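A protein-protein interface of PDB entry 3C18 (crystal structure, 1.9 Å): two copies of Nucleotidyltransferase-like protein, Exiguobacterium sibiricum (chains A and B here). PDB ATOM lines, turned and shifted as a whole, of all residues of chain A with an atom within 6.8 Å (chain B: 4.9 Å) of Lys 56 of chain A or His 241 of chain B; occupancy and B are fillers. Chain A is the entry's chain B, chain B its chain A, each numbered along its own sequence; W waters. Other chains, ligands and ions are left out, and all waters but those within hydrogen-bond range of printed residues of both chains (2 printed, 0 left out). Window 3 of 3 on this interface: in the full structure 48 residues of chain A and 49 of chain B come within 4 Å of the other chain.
OE2 of Glu 245 of chain B sits at hydrogen-bond distance from OG1 of Thr 54 of chain A (3.1 Å).
OG1 of Thr 54 of chain A sits at hydrogen-bond distance from ND1 of His 241 of chain B (3.1 Å).
The backbone NH (N) of Thr 54 of chain A sits at hydrogen-bond distance from the backbone carbonyl oxygen (O) of Leu 69 of chain A.
O of Lys 56 of chain A sits at hydrogen-bond distance from N of Leu 67 of chain A (2.8 Å).
The side-chain hydroxyl of Tyr 13 of chain A lies within hydrogen-bond range of the side-chain amino group of Lys 56 of chain A (2.7 Å).
Among the printed residues, merely in contact across the chains: Val 55 of chain A with His 241 of chain B, His 57 of chain A with Met 240 of chain B, Thr 54 of chain A with Met 244 of chain B, Val 55 of chain A with Met 244 of chain B, Lys 56 of chain A with His 241 of chain B and Val 55 of chain A with Met 240 of chain B.
Of the printed residues of chain B, Thr 54 of chain A touches His 241, Met 244 and Glu 245.
Of the printed residues of chain B, Val 55 of chain A touches Met 240 (3.9 Å), His 241 (3.3 Å) and Met 244 (3.8 Å).
Lys 56 of chain A touches just one residue of chain B: His 241.
Printed residues of chain B within 4 Å of His 57 of chain A: Met 240.
Of the printed residues of chain A, Met 240 of chain B touches Val 55 and His 57.
Of chain A, only Thr 54 (3.1 Å), Val 55 (3.3 Å) and Lys 56 (3.9 Å) come within 4 Å of His 241 of chain B.
Of the printed residues of chain A, Glu 245 of chain B touches Thr 54.
The nearest residue of chain B that does not touch Lys 56 of chain A is Met 240 of chain B (4.7 Å).
Of the 13 printed residues of chain A, 4 touch a printed residue of chain B.
Hydrophobic or aromatic side chains of chain A that line the printed part of chain B: Val 55 and His 57.
Printed residues of chain B that touch a printed residue of chain A: Met 240, His 241, Met 244 and Glu 245.
No position is printed for both chains.
Of the 8 pairs that touch across the chains among the printed residues, none has its exchanged pair printed and touching as well.
Water W1 bridges O of His 57 of chain A (2.7 Å) and N of Met 240 of chain B (3.2 Å).
Water W2 lies within hydrogen-bond range of N of His 241 of chain B and N of His 57 of chain A.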
ATOM      1  N   TYR A  13     -27.197   1.886   6.356  1.00  0.00           N
ATOM      2  CA  TYR A  13     -26.557   2.454   5.155  1.00  0.00           C
ATOM      3  C   TYR A  13     -27.597   2.724   4.099  1.00  0.00           C
ATOM      4  O   TYR A  13     -27.622   3.788   3.479  1.00  0.00           O
ATOM      5  CB  TYR A  13     -25.427   1.568   4.632  1.00  0.00           C
ATOM      6  CG  TYR A  13     -24.276   1.523   5.599  1.00  0.00           C
ATOM      7  CD1 TYR A  13     -24.253   0.579   6.626  1.00  0.00           C
ATOM      8  CD2 TYR A  13     -23.253   2.450   5.546  1.00  0.00           C
ATOM      9  CE1 TYR A  13     -23.222   0.507   7.550  1.00  0.00           C
ATOM     10  CE2 TYR A  13     -22.194   2.371   6.458  1.00  0.00           C
ATOM     11  CZ  TYR A  13     -22.207   1.407   7.491  1.00  0.00           C
ATOM     12  OH  TYR A  13     -21.182   1.340   8.440  1.00  0.00           O
ATOM     13  N   ASP A  36     -12.216 -11.121   2.160  1.00  0.00           N
ATOM     14  CA  ASP A  36     -11.330 -10.736   3.274  1.00  0.00           C
ATOM     15  C   ASP A  36     -11.210 -11.819   4.346  1.00  0.00           C
ATOM     16  O   ASP A  36     -11.069 -11.552   5.562  1.00  0.00           O
ATOM     17  CB  ASP A  36     -11.868  -9.450   3.937  1.00  0.00           C
ATOM     18  CG  ASP A  36     -11.505  -8.186   3.164  1.00  0.00           C
ATOM     19  OD1 ASP A  36     -10.721  -8.295   2.221  1.00  0.00           O
ATOM     20  OD2 ASP A  36     -11.999  -7.074   3.489  1.00  0.00           O
ATOM     21  N   PHE A  38     -13.440 -13.516   5.419  1.00  0.00           N
ATOM     22  CA  PHE A  38     -14.734 -13.590   6.146  1.00  0.00           C
ATOM     23  C   PHE A  38     -15.800 -14.282   5.322  1.00  0.00           C
ATOM     24  O   PHE A  38     -15.552 -14.690   4.206  1.00  0.00           O
ATOM     25  CB  PHE A  38     -15.236 -12.220   6.581  1.00  0.00           C
ATOM     26  CG  PHE A  38     -14.495 -11.653   7.759  1.00  0.00           C
ATOM     27  CD1 PHE A  38     -13.560 -12.421   8.423  1.00  0.00           C
ATOM     28  CD2 PHE A  38     -14.817 -10.392   8.290  1.00  0.00           C
ATOM     29  CE1 PHE A  38     -12.900 -11.915   9.542  1.00  0.00           C
ATOM     30  CE2 PHE A  38     -14.156  -9.892   9.404  1.00  0.00           C
ATOM     31  CZ  PHE A  38     -13.204 -10.641  10.019  1.00  0.00           C
ATOM     32  N   THR A  54     -13.046   3.116   3.052  1.00  0.00           N
ATOM     33  CA  THR A  54     -12.744   2.541   4.372  1.00  0.00           C
ATOM     34  C   THR A  54     -13.366   1.161   4.580  1.00  0.00           C
ATOM     35  O   THR A  54     -14.124   0.661   3.727  1.00  0.00           O
ATOM     36  CB  THR A  54     -13.140   3.522   5.490  1.00  0.00           C
ATOM     37  OG1 THR A  54     -12.621   3.034   6.725  1.00  0.00           O
ATOM     38  CG2 THR A  54     -14.687   3.725   5.522  1.00  0.00           C
ATOM     39  N   VAL A  55     -12.974   0.508   5.681  1.00  0.00           N
ATOM     40  CA  VAL A  55     -13.385  -0.854   5.988  1.00  0.00           C
ATOM     41  C   VAL A  55     -13.833  -0.982   7.427  1.00  0.00           C
ATOM     42  O   VAL A  55     -13.243  -0.409   8.303  1.00  0.00           O
ATOM     43  CB  VAL A  55     -12.272  -1.894   5.764  1.00  0.00           C
ATOM     44  CG1 VAL A  55     -12.793  -3.316   6.046  1.00  0.00           C
ATOM     45  CG2 VAL A  55     -11.731  -1.806   4.366  1.00  0.00           C
ATOM     46  N   LYS A  56     -14.906  -1.736   7.607  1.00  0.00           N
ATOM     47  CA  LYS A  56     -15.467  -2.075   8.936  1.00  0.00           C
ATOM     48  C   LYS A  56     -15.628  -3.642   8.993  1.00  0.00           C
ATOM     49  O   LYS A  56     -15.960  -4.252   8.029  1.00  0.00           O
ATOM     50  CB  LYS A  56     -16.807  -1.399   9.141  1.00  0.00           C
ATOM     51  CG  LYS A  56     -16.778   0.106   8.810  1.00  0.00           C
ATOM     52  CD  LYS A  56     -18.101   0.809   9.102  1.00  0.00           C
ATOM     53  CE  LYS A  56     -18.089   2.268   8.620  1.00  0.00           C
ATOM     54  NZ  LYS A  56     -19.234   3.065   9.209  1.00  0.00           N
ATOM     55  N   HIS A  57     -15.383  -4.225  10.158  1.00  0.00           N
ATOM     56  CA  HIS A  57     -15.508  -5.673  10.414  1.00  0.00           C
ATOM     57  C   HIS A  57     -16.460  -5.986  11.548  1.00  0.00           C
ATOM     58  O   HIS A  57     -16.366  -5.432  12.647  1.00  0.00           O
ATOM     59  CB  HIS A  57     -14.189  -6.257  10.834  1.00  0.00           C
ATOM     60  CG  HIS A  57     -13.198  -6.353   9.735  1.00  0.00           C
ATOM     61  ND1 HIS A  57     -11.888  -6.709   9.960  1.00  0.00           N
ATOM     62  CD2 HIS A  57     -13.315  -6.171   8.400  1.00  0.00           C
ATOM     63  CE1 HIS A  57     -11.233  -6.738   8.812  1.00  0.00           C
ATOM     64  NE2 HIS A  57     -12.076  -6.422   7.846  1.00  0.00           N
ATOM     65  N   TYR A  58     -17.352  -6.908  11.261  1.00  0.00           N
ATOM     66  CA  TYR A  58     -18.395  -7.336  12.172  1.00  0.00           C
ATOM     67  C   TYR A  58     -18.508  -8.830  12.258  1.00  0.00           C
ATOM     68  O   TYR A  58     -18.063  -9.557  11.403  1.00  0.00           O
ATOM     69  CB  TYR A  58     -19.774  -6.867  11.677  1.00  0.00           C
ATOM     70  CG  TYR A  58     -19.883  -5.388  11.334  1.00  0.00           C
ATOM     71  CD1 TYR A  58     -20.013  -4.429  12.316  1.00  0.00           C
ATOM     72  CD2 TYR A  58     -19.785  -4.963  10.019  1.00  0.00           C
ATOM     73  CE1 TYR A  58     -20.067  -3.076  11.977  1.00  0.00           C
ATOM     74  CE2 TYR A  58     -19.864  -3.646   9.683  1.00  0.00           C
ATOM     75  CZ  TYR A  58     -20.002  -2.718  10.643  1.00  0.00           C
ATOM     76  OH  TYR A  58     -20.072  -1.414  10.263  1.00  0.00           O
ATOM     77  N   VAL A  65     -18.556 -10.576   8.852  1.00  0.00           N
ATOM     78  CA  VAL A  65     -18.877  -9.673   7.727  1.00  0.00           C
ATOM     79  C   VAL A  65     -17.851  -8.567   7.620  1.00  0.00           C
ATOM     80  O   VAL A  65     -17.525  -7.945   8.593  1.00  0.00           O
ATOM     81  CB  VAL A  65     -20.283  -9.041   7.893  1.00  0.00           C
ATOM     82  CG1 VAL A  65     -20.649  -8.132   6.639  1.00  0.00           C
ATOM     83  CG2 VAL A  65     -21.367 -10.140   8.099  1.00  0.00           C
ATOM     84  N   SER A  66     -17.285  -8.424   6.432  1.00  0.00           N
ATOM     85  CA  SER A  66     -16.430  -7.293   6.095  1.00  0.00           C
ATOM     86  C   SER A  66     -17.164  -6.317   5.202  1.00  0.00           C
ATOM     87  O   SER A  66     -17.715  -6.674   4.182  1.00  0.00           O
ATOM     88  CB  SER A  66     -15.169  -7.741   5.395  1.00  0.00           C
ATOM     89  OG  SER A  66     -14.375  -6.619   5.039  1.00  0.00           O
ATOM     90  N   LEU A  67     -17.182  -5.067   5.627  1.00  0.00           N
ATOM     91  CA  LEU A  67     -17.882  -4.006   4.894  1.00  0.00           C
ATOM     92  C   LEU A  67     -16.920  -2.996   4.328  1.00  0.00           C
ATOM     93  O   LEU A  67     -16.192  -2.343   5.036  1.00  0.00           O
ATOM     94  CB  LEU A  67     -18.876  -3.339   5.832  1.00  0.00           C
ATOM     95  CG  LEU A  67     -19.871  -2.349   5.219  1.00  0.00           C
ATOM     96  CD1 LEU A  67     -21.167  -2.277   6.029  1.00  0.00           C
ATOM     97  CD2 LEU A  67     -19.183  -0.977   5.074  1.00  0.00           C
ATOM     98  N   HIS A  68     -16.927  -2.874   3.022  1.00  0.00           N
ATOM     99  CA  HIS A  68     -16.092  -1.882   2.330  1.00  0.00           C
ATOM    100  C   HIS A  68     -16.959  -0.717   1.902  1.00  0.00           C
ATOM    101  O   HIS A  68     -17.895  -0.881   1.173  1.00  0.00           O
ATOM    102  CB  HIS A  68     -15.462  -2.475   1.098  1.00  0.00           C
ATOM    103  CG  HIS A  68     -14.285  -3.354   1.395  1.00  0.00           C
ATOM    104  ND1 HIS A  68     -13.029  -3.056   0.945  1.00  0.00           N
ATOM    105  CD2 HIS A  68     -14.172  -4.491   2.108  1.00  0.00           C
ATOM    106  CE1 HIS A  68     -12.187  -4.007   1.318  1.00  0.00           C
ATOM    107  NE2 HIS A  68     -12.842  -4.866   2.065  1.00  0.00           N
ATOM    108  N   LEU A  69     -16.602   0.457   2.374  1.00  0.00           N
ATOM    109  CA  LEU A  69     -17.390   1.657   2.100  1.00  0.00           C
ATOM    110  C   LEU A  69     -16.524   2.514   1.172  1.00  0.00           C
ATOM    111  O   LEU A  69     -15.398   2.900   1.521  1.00  0.00           O
ATOM    112  CB  LEU A  69     -17.686   2.401   3.418  1.00  0.00           C
ATOM    113  CG  LEU A  69     -18.531   3.679   3.418  1.00  0.00           C
ATOM    114  CD1 LEU A  69     -19.935   3.368   2.890  1.00  0.00           C
ATOM    115  CD2 LEU A  69     -18.553   4.314   4.810  1.00  0.00           C
ATOM    116  N   THR B 239     -10.978  -1.527  16.747  1.00  0.00           N
ATOM    117  CA  THR B 239     -11.840  -2.079  15.680  1.00  0.00           C
ATOM    118  C   THR B 239     -11.077  -1.868  14.357  1.00  0.00           C
ATOM    119  O   THR B 239     -10.184  -1.057  14.278  1.00  0.00           O
ATOM    120  CB  THR B 239     -13.185  -1.355  15.591  1.00  0.00           C
ATOM    121  OG1 THR B 239     -12.957   0.009  15.234  1.00  0.00           O
ATOM    122  CG2 THR B 239     -13.936  -1.414  16.890  1.00  0.00           C
ATOM    123  N   MET B 240     -11.450  -2.584  13.308  1.00  0.00           N
ATOM    124  CA  MET B 240     -10.822  -2.389  12.003  1.00  0.00           C
ATOM    125  C   MET B 240     -11.021  -0.969  11.546  1.00  0.00           C
ATOM    126  O   MET B 240     -10.113  -0.325  11.058  1.00  0.00           O
ATOM    127  CB  MET B 240     -11.418  -3.339  10.950  1.00  0.00           C
ATOM    128  CG  MET B 240     -10.858  -3.190   9.545  1.00  0.00           C
ATOM    129  SD  MET B 240      -8.896  -3.263   9.467  1.00  0.00           S
ATOM    130  CE  MET B 240      -8.500  -5.098   9.965  1.00  0.00           C
ATOM    131  N   HIS B 241     -12.232  -0.476  11.704  1.00  0.00           N
ATOM    132  CA  HIS B 241     -12.534   0.917  11.269  1.00  0.00           C
ATOM    133  C   HIS B 241     -11.641   1.923  11.964  1.00  0.00           C
ATOM    134  O   HIS B 241     -11.131   2.866  11.368  1.00  0.00           O
ATOM    135  CB  HIS B 241     -14.008   1.260  11.442  1.00  0.00           C
ATOM    136  CG  HIS B 241     -14.403   2.545  10.795  1.00  0.00           C
ATOM    137  ND1 HIS B 241     -14.109   2.822   9.479  1.00  0.00           N
ATOM    138  CD2 HIS B 241     -15.095   3.610  11.266  1.00  0.00           C
ATOM    139  CE1 HIS B 241     -14.581   4.018   9.178  1.00  0.00           C
ATOM    140  NE2 HIS B 241     -15.192   4.514  10.239  1.00  0.00           N
ATOM    141  N   GLU B 242     -11.397   1.685  13.223  1.00  0.00           N
ATOM    142  CA  GLU B 242     -10.545   2.582  14.017  1.00  0.00           C
ATOM    143  C   GLU B 242      -9.104   2.583  13.478  1.00  0.00           C
ATOM    144  O   GLU B 242      -8.411   3.591  13.434  1.00  0.00           O
ATOM    145  CB  GLU B 242     -10.559   2.175  15.475  1.00  0.00           C
ATOM    146  CG  GLU B 242     -11.848   2.590  16.182  1.00  0.00           C
ATOM    147  CD  GLU B 242     -11.949   2.072  17.622  1.00  0.00           C
ATOM    148  OE1 GLU B 242     -11.210   1.146  18.003  1.00  0.00           O
ATOM    149  OE2 GLU B 242     -12.816   2.583  18.379  1.00  0.00           O
ATOM    150  N   LEU B 243      -8.653   1.414  13.119  1.00  0.00           N
ATOM    151  CA  LEU B 243      -7.307   1.238  12.542  1.00  0.00           C
ATOM    152  C   LEU B 243      -7.231   1.945  11.191  1.00  0.00           C
ATOM    153  O   LEU B 243      -6.276   2.672  10.879  1.00  0.00           O
ATOM    154  CB  LEU B 243      -6.966  -0.252  12.373  1.00  0.00           C
ATOM    155  CG  LEU B 243      -6.567  -1.123  13.576  1.00  0.00           C
ATOM    156  CD1 LEU B 243      -6.429  -2.582  13.166  1.00  0.00           C
ATOM    157  CD2 LEU B 243      -5.273  -0.658  14.219  1.00  0.00           C
ATOM    158  N   MET B 244      -8.270   1.753  10.400  1.00  0.00           N
ATOM    159  CA  MET B 244      -8.338   2.355   9.072  1.00  0.00           C
ATOM    160  C   MET B 244      -8.382   3.855   9.094  1.00  0.00           C
ATOM    161  O   MET B 244      -8.004   4.494   8.109  1.00  0.00           O
ATOM    162  CB  MET B 244      -9.527   1.854   8.265  1.00  0.00           C
ATOM    163  CG  MET B 244      -9.468   0.412   7.932  1.00  0.00           C
ATOM    164  SD  MET B 244      -8.242  -0.066   6.508  1.00  0.00           S
ATOM    165  CE  MET B 244      -9.162   0.843   5.118  1.00  0.00           C
ATOM    166  N   GLU B 245      -8.858   4.405  10.206  1.00  0.00           N
ATOM    167  CA  GLU B 245      -9.079   5.828  10.337  1.00  0.00           C
ATOM    168  C   GLU B 245      -7.934   6.529  11.040  1.00  0.00           C
ATOM    169  O   GLU B 245      -7.870   7.727  11.071  1.00  0.00           O
ATOM    170  CB  GLU B 245     -10.364   6.128  11.116  1.00  0.00           C
ATOM    171  CG  GLU B 245     -11.661   5.787  10.380  1.00  0.00           C
ATOM    172  CD  GLU B 245     -11.766   6.450   8.996  1.00  0.00           C
ATOM    173  OE1 GLU B 245     -11.890   7.684   9.017  1.00  0.00           O
ATOM    174  OE2 GLU B 245     -11.762   5.740   7.930  1.00  0.00           O
HETATM  175  O   HOH W   1     -14.176  -4.251  13.647  1.00  0.00           O
HETATM  176  O   HOH W   2     -14.911  -1.839  12.247  1.00  0.00           O
